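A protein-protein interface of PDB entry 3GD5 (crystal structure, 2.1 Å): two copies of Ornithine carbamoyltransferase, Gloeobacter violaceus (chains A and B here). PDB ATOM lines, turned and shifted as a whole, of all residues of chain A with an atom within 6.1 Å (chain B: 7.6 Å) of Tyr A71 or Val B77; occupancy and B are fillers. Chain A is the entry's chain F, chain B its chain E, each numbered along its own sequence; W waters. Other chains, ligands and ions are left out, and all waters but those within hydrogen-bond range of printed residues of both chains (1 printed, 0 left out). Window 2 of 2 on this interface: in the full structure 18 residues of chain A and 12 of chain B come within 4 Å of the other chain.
Water W1 bridges O of Gly B48 and OE1 of Gln A72.
Tyr A71 touches just these residues of chain B: Gln B76 (3.1 Å) and Val B77 (3.4 Å).
Val B77 touches one residue of chain A.
Of the printed residues of chain B, Thr A67 touches Ile B78 (3.2 Å).
Of the printed residues of chain B, Val A68 touches Ile B78 (3.6 Å).
The nearest printed residue of chain A that does not touch Ile B78 is Tyr A71 (4.1 Å).
OE1 of Gln B76 lies within hydrogen-bond range of OH of Tyr A71 (3.1 Å).
The side-chain amide oxygen (OE1) of Gln A76 lies within hydrogen-bond range of the side-chain amide nitrogen (NE2) of Gln B76 (3.4 Å).
O of Val B77 lies within hydrogen-bond range of OH of Tyr A71 (3.4 Å).
O of Leu B51 lies within hydrogen-bond range of N of Ile B78, 2.9 Å away.
N of Leu B53 lies within hydrogen-bond range of O of Ile B78, at 2.7 Å.
N of Leu B51 sits at hydrogen-bond distance from O of Gln B76, at 2.8 Å.
The backbone NH (N) of Gln B76 sits at hydrogen-bond distance from the backbone carbonyl oxygen (O) of Lys B49 (2.8 Å).
Among the printed residues, pairs that only touch across the chains: Thr A67 with Ile B78 and Val A68 with Ile B78.
Tyr A71 touches Gln B76, but with the chains exchanged Gln A76 does not touch Tyr B71 (6.1 Å).
Tyr A71 touches Val B77, but with the chains exchanged Val A77 does not touch Tyr B71 (7.6 Å).
Gln A76 touches its own counterpart, Gln B76.
Positions printed for both chains: 66, 67, 68, 69, 70, 71, 75, 76 and 77.
Printed residues of chain A that touch a printed residue of chain B: Thr A67, Val A68, Tyr A71 and Gln A76.
Hydrophobic or aromatic side chains of chain A within 4 Å of the printed part of chain B: Val A68 and Tyr A71.
Printed residues of chain B that touch a printed residue of chain A: Gln B76, Val B77 and Ile B78.
Hydrophobic or aromatic side chains of chain B within 4 Å of the printed part of chain A: Ile B78.
Among the printed residues, 5 pairs touch across the chains.
Among the printed residues, no Asp or Glu carboxylate lies within 4 Å of a Lys or Arg side-chain nitrogen of the other chain.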
ATOM      1  N   PHE A  66      23.574  39.291  15.486  1.00  0.00           N
ATOM      2  CA  PHE A  66      24.159  39.247  16.828  1.00  0.00           C
ATOM      3  C   PHE A  66      25.152  38.080  16.973  1.00  0.00           C
ATOM      4  O   PHE A  66      26.196  38.213  17.616  1.00  0.00           O
ATOM      5  CB  PHE A  66      23.061  39.112  17.898  1.00  0.00           C
ATOM      6  CG  PHE A  66      22.600  40.432  18.477  1.00  0.00           C
ATOM      7  CD1 PHE A  66      23.403  41.136  19.374  1.00  0.00           C
ATOM      8  CD2 PHE A  66      21.379  40.978  18.105  1.00  0.00           C
ATOM      9  CE1 PHE A  66      22.995  42.371  19.889  1.00  0.00           C
ATOM     10  CE2 PHE A  66      20.958  42.221  18.614  1.00  0.00           C
ATOM     11  CZ  PHE A  66      21.764  42.915  19.503  1.00  0.00           C
ATOM     12  N   THR A  67      24.831  36.940  16.370  1.00  0.00           N
ATOM     13  CA  THR A  67      25.707  35.782  16.488  1.00  0.00           C
ATOM     14  C   THR A  67      27.021  35.952  15.744  1.00  0.00           C
ATOM     15  O   THR A  67      28.086  35.621  16.281  1.00  0.00           O
ATOM     16  CB  THR A  67      25.005  34.497  16.024  1.00  0.00           C
ATOM     17  OG1 THR A  67      25.932  33.399  16.069  1.00  0.00           O
ATOM     18  CG2 THR A  67      24.496  34.655  14.617  1.00  0.00           C
ATOM     19  N   VAL A  68      26.961  36.465  14.516  1.00  0.00           N
ATOM     20  CA  VAL A  68      28.181  36.683  13.744  1.00  0.00           C
ATOM     21  C   VAL A  68      29.020  37.753  14.450  1.00  0.00           C
ATOM     22  O   VAL A  68      30.249  37.694  14.445  1.00  0.00           O
ATOM     23  CB  VAL A  68      27.872  37.150  12.297  1.00  0.00           C
ATOM     24  CG1 VAL A  68      29.166  37.521  11.574  1.00  0.00           C
ATOM     25  CG2 VAL A  68      27.165  36.044  11.528  1.00  0.00           C
ATOM     26  N   ALA A  69      28.356  38.722  15.075  1.00  0.00           N
ATOM     27  CA  ALA A  69      29.073  39.783  15.773  1.00  0.00           C
ATOM     28  C   ALA A  69      29.932  39.222  16.912  1.00  0.00           C
ATOM     29  O   ALA A  69      31.092  39.607  17.075  1.00  0.00           O
ATOM     30  CB  ALA A  69      28.093  40.817  16.305  1.00  0.00           C
ATOM     31  N   MET A  70      29.367  38.314  17.700  1.00  0.00           N
ATOM     32  CA  MET A  70      30.118  37.725  18.802  1.00  0.00           C
ATOM     33  C   MET A  70      31.222  36.825  18.257  1.00  0.00           C
ATOM     34  O   MET A  70      32.364  36.868  18.733  1.00  0.00           O
ATOM     35  CB  MET A  70      29.197  36.907  19.712  1.00  0.00           C
ATOM     36  CG  MET A  70      29.915  36.395  20.952  1.00  0.00           C
ATOM     37  SD  MET A  70      30.565  37.760  21.965  1.00  0.00           S
ATOM     38  CE  MET A  70      30.354  37.071  23.605  1.00  0.00           C
ATOM     39  N   TYR A  71      30.891  36.013  17.255  1.00  0.00           N
ATOM     40  CA  TYR A  71      31.876  35.113  16.660  1.00  0.00           C
ATOM     41  C   TYR A  71      33.114  35.885  16.186  1.00  0.00           C
ATOM     42  O   TYR A  71      34.252  35.488  16.460  1.00  0.00           O
ATOM     43  CB  TYR A  71      31.273  34.351  15.466  1.00  0.00           C
ATOM     44  CG  TYR A  71      30.312  33.230  15.820  1.00  0.00           C
ATOM     45  CD1 TYR A  71      30.199  32.762  17.129  1.00  0.00           C
ATOM     46  CD2 TYR A  71      29.537  32.611  14.830  1.00  0.00           C
ATOM     47  CE1 TYR A  71      29.335  31.706  17.443  1.00  0.00           C
ATOM     48  CE2 TYR A  71      28.680  31.556  15.135  1.00  0.00           C
ATOM     49  CZ  TYR A  71      28.586  31.113  16.440  1.00  0.00           C
ATOM     50  OH  TYR A  71      27.747  30.075  16.753  1.00  0.00           O
ATOM     51  N   GLN A  72      32.894  36.994  15.483  1.00  0.00           N
ATOM     52  CA  GLN A  72      34.017  37.774  14.990  1.00  0.00           C
ATOM     53  C   GLN A  72      34.804  38.407  16.129  1.00  0.00           C
ATOM     54  O   GLN A  72      35.921  38.881  15.922  1.00  0.00           O
ATOM     55  CB  GLN A  72      33.546  38.825  13.977  1.00  0.00           C
ATOM     56  CG  GLN A  72      33.091  38.187  12.662  1.00  0.00           C
ATOM     57  CD  GLN A  72      32.833  39.194  11.559  1.00  0.00           C
ATOM     58  OE1 GLN A  72      32.558  38.818  10.415  1.00  0.00           O
ATOM     59  NE2 GLN A  72      32.916  40.481  11.894  1.00  0.00           N
ATOM     60  N   LEU A  73      34.232  38.396  17.333  1.00  0.00           N
ATOM     61  CA  LEU A  73      34.918  38.938  18.500  1.00  0.00           C
ATOM     62  C   LEU A  73      35.633  37.818  19.268  1.00  0.00           C
ATOM     63  O   LEU A  73      36.273  38.070  20.290  1.00  0.00           O
ATOM     64  CB  LEU A  73      33.933  39.640  19.441  1.00  0.00           C
ATOM     65  CG  LEU A  73      33.470  41.041  19.035  1.00  0.00           C
ATOM     66  CD1 LEU A  73      32.536  41.609  20.094  1.00  0.00           C
ATOM     67  CD2 LEU A  73      34.688  41.934  18.861  1.00  0.00           C
ATOM     68  N   GLY A  74      35.512  36.584  18.780  1.00  0.00           N
ATOM     69  CA  GLY A  74      36.161  35.462  19.443  1.00  0.00           C
ATOM     70  C   GLY A  74      35.358  34.829  20.573  1.00  0.00           C
ATOM     71  O   GLY A  74      35.870  33.986  21.311  1.00  0.00           O
ATOM     72  N   GLY A  75      34.096  35.227  20.713  1.00  0.00           N
ATOM     73  CA  GLY A  75      33.263  34.666  21.765  1.00  0.00           C
ATOM     74  C   GLY A  75      32.296  33.613  21.256  1.00  0.00           C
ATOM     75  O   GLY A  75      32.250  33.330  20.059  1.00  0.00           O
ATOM     76  N   GLN A  76      31.533  33.016  22.167  1.00  0.00           N
ATOM     77  CA  GLN A  76      30.553  32.001  21.792  1.00  0.00           C
ATOM     78  C   GLN A  76      29.136  32.502  22.080  1.00  0.00           C
ATOM     79  O   GLN A  76      28.935  33.446  22.862  1.00  0.00           O
ATOM     80  CB  GLN A  76      30.815  30.700  22.558  1.00  0.00           C
ATOM     81  CG  GLN A  76      31.925  29.841  21.963  1.00  0.00           C
ATOM     82  CD  GLN A  76      31.498  29.159  20.671  1.00  0.00           C
ATOM     83  OE1 GLN A  76      31.009  29.804  19.748  1.00  0.00           O
ATOM     84  NE2 GLN A  76      31.681  27.847  20.607  1.00  0.00           N
ATOM     85  N   VAL A  77      28.150  31.887  21.439  1.00  0.00           N
ATOM     86  CA  VAL A  77      26.784  32.310  21.666  1.00  0.00           C
ATOM     87  C   VAL A  77      25.861  31.113  21.819  1.00  0.00           C
ATOM     88  O   VAL A  77      26.124  30.038  21.281  1.00  0.00           O
ATOM     89  CB  VAL A  77      26.285  33.278  20.532  1.00  0.00           C
ATOM     90  CG1 VAL A  77      27.461  33.776  19.715  1.00  0.00           C
ATOM     91  CG2 VAL A  77      25.247  32.623  19.663  1.00  0.00           C
ATOM     92  N   HIS B  47      38.787  29.201   9.094  1.00  0.00           N
ATOM     93  CA  HIS B  47      38.742  29.994  10.305  1.00  0.00           C
ATOM     94  C   HIS B  47      38.262  31.397   9.960  1.00  0.00           C
ATOM     95  O   HIS B  47      38.652  31.955   8.941  1.00  0.00           O
ATOM     96  CB  HIS B  47      40.125  30.053  10.957  1.00  0.00           C
ATOM     97  CG  HIS B  47      40.194  30.999  12.113  1.00  0.00           C
ATOM     98  ND1 HIS B  47      40.418  32.350  11.955  1.00  0.00           N
ATOM     99  CD2 HIS B  47      40.003  30.801  13.438  1.00  0.00           C
ATOM    100  CE1 HIS B  47      40.360  32.943  13.134  1.00  0.00           C
ATOM    101  NE2 HIS B  47      40.110  32.027  14.051  1.00  0.00           N
ATOM    102  N   GLY B  48      37.406  31.956  10.811  1.00  0.00           N
ATOM    103  CA  GLY B  48      36.877  33.285  10.566  1.00  0.00           C
ATOM    104  C   GLY B  48      35.657  33.261   9.668  1.00  0.00           C
ATOM    105  O   GLY B  48      35.040  34.296   9.421  1.00  0.00           O
ATOM    106  N   LYS B  49      35.294  32.080   9.179  1.00  0.00           N
ATOM    107  CA  LYS B  49      34.141  31.957   8.296  1.00  0.00           C
ATOM    108  C   LYS B  49      32.945  31.365   9.026  1.00  0.00           C
ATOM    109  O   LYS B  49      33.095  30.615   9.992  1.00  0.00           O
ATOM    110  CB  LYS B  49      34.470  31.067   7.093  1.00  0.00           C
ATOM    111  CG  LYS B  49      35.737  31.426   6.349  1.00  0.00           C
ATOM    112  CD  LYS B  49      35.591  32.689   5.537  1.00  0.00           C
ATOM    113  CE  LYS B  49      36.883  32.966   4.753  1.00  0.00           C
ATOM    114  NZ  LYS B  49      37.255  31.839   3.840  1.00  0.00           N
ATOM    115  N   VAL B  50      31.755  31.699   8.542  1.00  0.00           N
ATOM    116  CA  VAL B  50      30.521  31.221   9.137  1.00  0.00           C
ATOM    117  C   VAL B  50      29.620  30.609   8.084  1.00  0.00           C
ATOM    118  O   VAL B  50      29.412  31.191   7.022  1.00  0.00           O
ATOM    119  CB  VAL B  50      29.749  32.364   9.817  1.00  0.00           C
ATOM    120  CG1 VAL B  50      28.434  31.837  10.388  1.00  0.00           C
ATOM    121  CG2 VAL B  50      30.609  32.986  10.897  1.00  0.00           C
ATOM    122  N   LEU B  51      29.075  29.436   8.387  1.00  0.00           N
ATOM    123  CA  LEU B  51      28.186  28.747   7.465  1.00  0.00           C
ATOM    124  C   LEU B  51      26.769  28.919   7.973  1.00  0.00           C
ATOM    125  O   LEU B  51      26.481  28.595   9.128  1.00  0.00           O
ATOM    126  CB  LEU B  51      28.508  27.248   7.423  1.00  0.00           C
ATOM    127  CG  LEU B  51      28.135  26.386   6.202  1.00  0.00           C
ATOM    128  CD1 LEU B  51      27.773  24.990   6.693  1.00  0.00           C
ATOM    129  CD2 LEU B  51      26.986  26.991   5.402  1.00  0.00           C
ATOM    130  N   GLY B  52      25.887  29.428   7.119  1.00  0.00           N
ATOM    131  CA  GLY B  52      24.504  29.589   7.517  1.00  0.00           C
ATOM    132  C   GLY B  52      23.731  28.365   7.057  1.00  0.00           C
ATOM    133  O   GLY B  52      23.867  27.942   5.914  1.00  0.00           O
ATOM    134  N   LEU B  53      22.940  27.771   7.941  1.00  0.00           N
ATOM    135  CA  LEU B  53      22.152  26.600   7.573  1.00  0.00           C
ATOM    136  C   LEU B  53      20.703  27.030   7.469  1.00  0.00           C
ATOM    137  O   LEU B  53      20.054  27.269   8.479  1.00  0.00           O
ATOM    138  CB  LEU B  53      22.279  25.500   8.632  1.00  0.00           C
ATOM    139  CG  LEU B  53      23.686  25.027   9.003  1.00  0.00           C
ATOM    140  CD1 LEU B  53      23.575  23.860   9.979  1.00  0.00           C
ATOM    141  CD2 LEU B  53      24.458  24.610   7.763  1.00  0.00           C
ATOM    142  N   ARG B  63      21.751  18.513   9.393  1.00  0.00           N
ATOM    143  CA  ARG B  63      22.278  19.621  10.170  1.00  0.00           C
ATOM    144  C   ARG B  63      23.571  19.220  10.867  1.00  0.00           C
ATOM    145  O   ARG B  63      24.592  19.882  10.721  1.00  0.00           O
ATOM    146  CB  ARG B  63      21.249  20.090  11.205  1.00  0.00           C
ATOM    147  CG  ARG B  63      21.720  21.287  12.034  1.00  0.00           C
ATOM    148  CD  ARG B  63      20.547  22.098  12.532  1.00  0.00           C
ATOM    149  NE  ARG B  63      19.723  21.313  13.433  1.00  0.00           N
ATOM    150  CZ  ARG B  63      20.078  21.010  14.674  1.00  0.00           C
ATOM    151  NH1 ARG B  63      21.237  21.437  15.146  1.00  0.00           N
ATOM    152  NH2 ARG B  63      19.283  20.268  15.432  1.00  0.00           N
ATOM    153  N   PHE B  66      26.674  18.736   8.528  1.00  0.00           N
ATOM    154  CA  PHE B  66      27.203  19.970   7.974  1.00  0.00           C
ATOM    155  C   PHE B  66      27.887  20.769   9.086  1.00  0.00           C
ATOM    156  O   PHE B  66      28.977  21.300   8.885  1.00  0.00           O
ATOM    157  CB  PHE B  66      26.090  20.818   7.340  1.00  0.00           C
ATOM    158  CG  PHE B  66      25.874  20.559   5.867  1.00  0.00           C
ATOM    159  CD1 PHE B  66      26.729  21.104   4.920  1.00  0.00           C
ATOM    160  CD2 PHE B  66      24.816  19.768   5.431  1.00  0.00           C
ATOM    161  CE1 PHE B  66      26.539  20.867   3.559  1.00  0.00           C
ATOM    162  CE2 PHE B  66      24.618  19.524   4.072  1.00  0.00           C
ATOM    163  CZ  PHE B  66      25.481  20.074   3.135  1.00  0.00           C
ATOM    164  N   THR B  67      27.259  20.842  10.260  1.00  0.00           N
ATOM    165  CA  THR B  67      27.838  21.609  11.358  1.00  0.00           C
ATOM    166  C   THR B  67      29.169  21.039  11.843  1.00  0.00           C
ATOM    167  O   THR B  67      30.125  21.790  12.039  1.00  0.00           O
ATOM    168  CB  THR B  67      26.830  21.777  12.552  1.00  0.00           C
ATOM    169  OG1 THR B  67      27.516  22.311  13.698  1.00  0.00           O
ATOM    170  CG2 THR B  67      26.209  20.471  12.925  1.00  0.00           C
ATOM    171  N   VAL B  68      29.261  19.724  12.023  1.00  0.00           N
ATOM    172  CA  VAL B  68      30.534  19.154  12.453  1.00  0.00           C
ATOM    173  C   VAL B  68      31.570  19.340  11.342  1.00  0.00           C
ATOM    174  O   VAL B  68      32.752  19.578  11.613  1.00  0.00           O
ATOM    175  CB  VAL B  68      30.412  17.658  12.794  1.00  0.00           C
ATOM    176  CG1 VAL B  68      31.798  17.084  13.120  1.00  0.00           C
ATOM    177  CG2 VAL B  68      29.482  17.476  13.987  1.00  0.00           C
ATOM    178  N   ALA B  69      31.126  19.250  10.091  1.00  0.00           N
ATOM    179  CA  ALA B  69      32.029  19.428   8.948  1.00  0.00           C
ATOM    180  C   ALA B  69      32.697  20.807   8.984  1.00  0.00           C
ATOM    181  O   ALA B  69      33.900  20.933   8.752  1.00  0.00           O
ATOM    182  CB  ALA B  69      31.263  19.255   7.634  1.00  0.00           C
ATOM    183  N   MET B  70      31.912  21.843   9.264  1.00  0.00           N
ATOM    184  CA  MET B  70      32.454  23.197   9.330  1.00  0.00           C
ATOM    185  C   MET B  70      33.340  23.350  10.572  1.00  0.00           C
ATOM    186  O   MET B  70      34.381  24.014  10.527  1.00  0.00           O
ATOM    187  CB  MET B  70      31.319  24.221   9.374  1.00  0.00           C
ATOM    188  CG  MET B  70      31.799  25.668   9.322  1.00  0.00           C
ATOM    189  SD  MET B  70      32.685  26.043   7.803  1.00  0.00           S
ATOM    190  CE  MET B  70      32.324  27.784   7.563  1.00  0.00           C
ATOM    191  N   TYR B  71      32.938  22.730  11.679  1.00  0.00           N
ATOM    192  CA  TYR B  71      33.727  22.825  12.905  1.00  0.00           C
ATOM    193  C   TYR B  71      35.132  22.238  12.713  1.00  0.00           C
ATOM    194  O   TYR B  71      36.122  22.803  13.176  1.00  0.00           O
ATOM    195  CB  TYR B  71      33.026  22.106  14.061  1.00  0.00           C
ATOM    196  CG  TYR B  71      31.832  22.827  14.665  1.00  0.00           C
ATOM    197  CD1 TYR B  71      31.571  24.165  14.373  1.00  0.00           C
ATOM    198  CD2 TYR B  71      30.978  22.173  15.554  1.00  0.00           C
ATOM    199  CE1 TYR B  71      30.490  24.828  14.948  1.00  0.00           C
ATOM    200  CE2 TYR B  71      29.895  22.831  16.138  1.00  0.00           C
ATOM    201  CZ  TYR B  71      29.655  24.155  15.830  1.00  0.00           C
ATOM    202  OH  TYR B  71      28.577  24.807  16.392  1.00  0.00           O
ATOM    203  N   GLY B  75      35.591  26.553  11.136  1.00  0.00           N
ATOM    204  CA  GLY B  75      34.620  27.613  10.910  1.00  0.00           C
ATOM    205  C   GLY B  75      33.481  27.568  11.912  1.00  0.00           C
ATOM    206  O   GLY B  75      33.436  26.679  12.764  1.00  0.00           O
ATOM    207  N   GLN B  76      32.567  28.529  11.829  1.00  0.00           N
ATOM    208  CA  GLN B  76      31.422  28.544  12.728  1.00  0.00           C
ATOM    209  C   GLN B  76      30.140  28.261  11.951  1.00  0.00           C
ATOM    210  O   GLN B  76      30.132  28.289  10.718  1.00  0.00           O
ATOM    211  CB  GLN B  76      31.321  29.879  13.461  1.00  0.00           C
ATOM    212  CG  GLN B  76      31.784  29.819  14.909  1.00  0.00           C
ATOM    213  CD  GLN B  76      31.036  28.765  15.725  1.00  0.00           C
ATOM    214  OE1 GLN B  76      29.903  28.382  15.400  1.00  0.00           O
ATOM    215  NE2 GLN B  76      31.663  28.304  16.801  1.00  0.00           N
ATOM    216  N   VAL B  77      29.058  27.994  12.676  1.00  0.00           N
ATOM    217  CA  VAL B  77      27.787  27.662  12.046  1.00  0.00           C
ATOM    218  C   VAL B  77      26.580  28.326  12.712  1.00  0.00           C
ATOM    219  O   VAL B  77      26.571  28.550  13.918  1.00  0.00           O
ATOM    220  CB  VAL B  77      27.584  26.122  12.066  1.00  0.00           C
ATOM    221  CG1 VAL B  77      26.306  25.744  11.350  1.00  0.00           C
ATOM    222  CG2 VAL B  77      28.780  25.438  11.425  1.00  0.00           C
ATOM    223  N   ILE B  78      25.568  28.636  11.907  1.00  0.00           N
ATOM    224  CA  ILE B  78      24.342  29.252  12.396  1.00  0.00           C
ATOM    225  C   ILE B  78      23.130  28.587  11.755  1.00  0.00           C
ATOM    226  O   ILE B  78      23.011  28.544  10.530  1.00  0.00           O
ATOM    227  CB  ILE B  78      24.266  30.753  12.060  1.00  0.00           C
ATOM    228  CG1 ILE B  78      25.480  31.483  12.615  1.00  0.00           C
ATOM    229  CG2 ILE B  78      22.988  31.345  12.659  1.00  0.00           C
ATOM    230  CD1 ILE B  78      25.557  32.927  12.173  1.00  0.00           C
ATOM    231  N   ASP B  79      22.232  28.076  12.589  1.00  0.00           N
ATOM    232  CA  ASP B  79      21.022  27.423  12.106  1.00  0.00           C
ATOM    233  C   ASP B  79      19.945  28.472  11.823  1.00  0.00           C
ATOM    234  O   ASP B  79      19.620  29.278  12.690  1.00  0.00           O
ATOM    235  CB  ASP B  79      20.509  26.424  13.150  1.00  0.00           C
ATOM    236  CG  ASP B  79      19.406  25.516  12.607  1.00  0.00           C
ATOM    237  OD1 ASP B  79      18.956  25.738  11.459  1.00  0.00           O
ATOM    238  OD2 ASP B  79      18.992  24.580  13.330  1.00  0.00           O
ATOM    239  N   LEU B  80      19.406  28.465  10.608  1.00  0.00           N
ATOM    240  CA  LEU B  80      18.358  29.407  10.218  1.00  0.00           C
ATOM    241  C   LEU B  80      17.151  28.679   9.634  1.00  0.00           C
ATOM    242  O   LEU B  80      16.755  27.619  10.119  1.00  0.00           O
ATOM    243  CB  LEU B  80      18.879  30.417   9.187  1.00  0.00           C
ATOM    244  CG  LEU B  80      19.988  31.402   9.571  1.00  0.00           C
ATOM    245  CD1 LEU B  80      19.785  31.855  11.010  1.00  0.00           C
ATOM    246  CD2 LEU B  80      21.344  30.752   9.421  1.00  0.00           C
ATOM    247  N   VAL B 104      27.031  36.086   6.669  1.00  0.00           N
ATOM    248  CA  VAL B 104      27.777  34.833   6.627  1.00  0.00           C
ATOM    249  C   VAL B 104      28.528  34.658   5.316  1.00  0.00           C
ATOM    250  O   VAL B 104      28.405  35.478   4.408  1.00  0.00           O
ATOM    251  CB  VAL B 104      26.845  33.626   6.857  1.00  0.00           C
ATOM    252  CG1 VAL B 104      26.171  33.743   8.233  1.00  0.00           C
ATOM    253  CG2 VAL B 104      25.803  33.560   5.751  1.00  0.00           C
ATOM    254  N   LEU B 308      32.558  22.235   1.341  1.00  0.00           N
ATOM    255  CA  LEU B 308      32.728  23.490   2.073  1.00  0.00           C
ATOM    256  C   LEU B 308      34.090  24.104   1.768  1.00  0.00           C
ATOM    257  O   LEU B 308      34.190  25.300   1.497  1.00  0.00           O
ATOM    258  CB  LEU B 308      32.561  23.269   3.591  1.00  0.00           C
ATOM    259  CG  LEU B 308      31.133  22.932   4.076  1.00  0.00           C
ATOM    260  CD1 LEU B 308      31.137  22.582   5.550  1.00  0.00           C
ATOM    261  CD2 LEU B 308      30.194  24.124   3.829  1.00  0.00           C
HETATM  262  O   HOH W   1      32.929  35.728  10.371  1.00  0.00           O
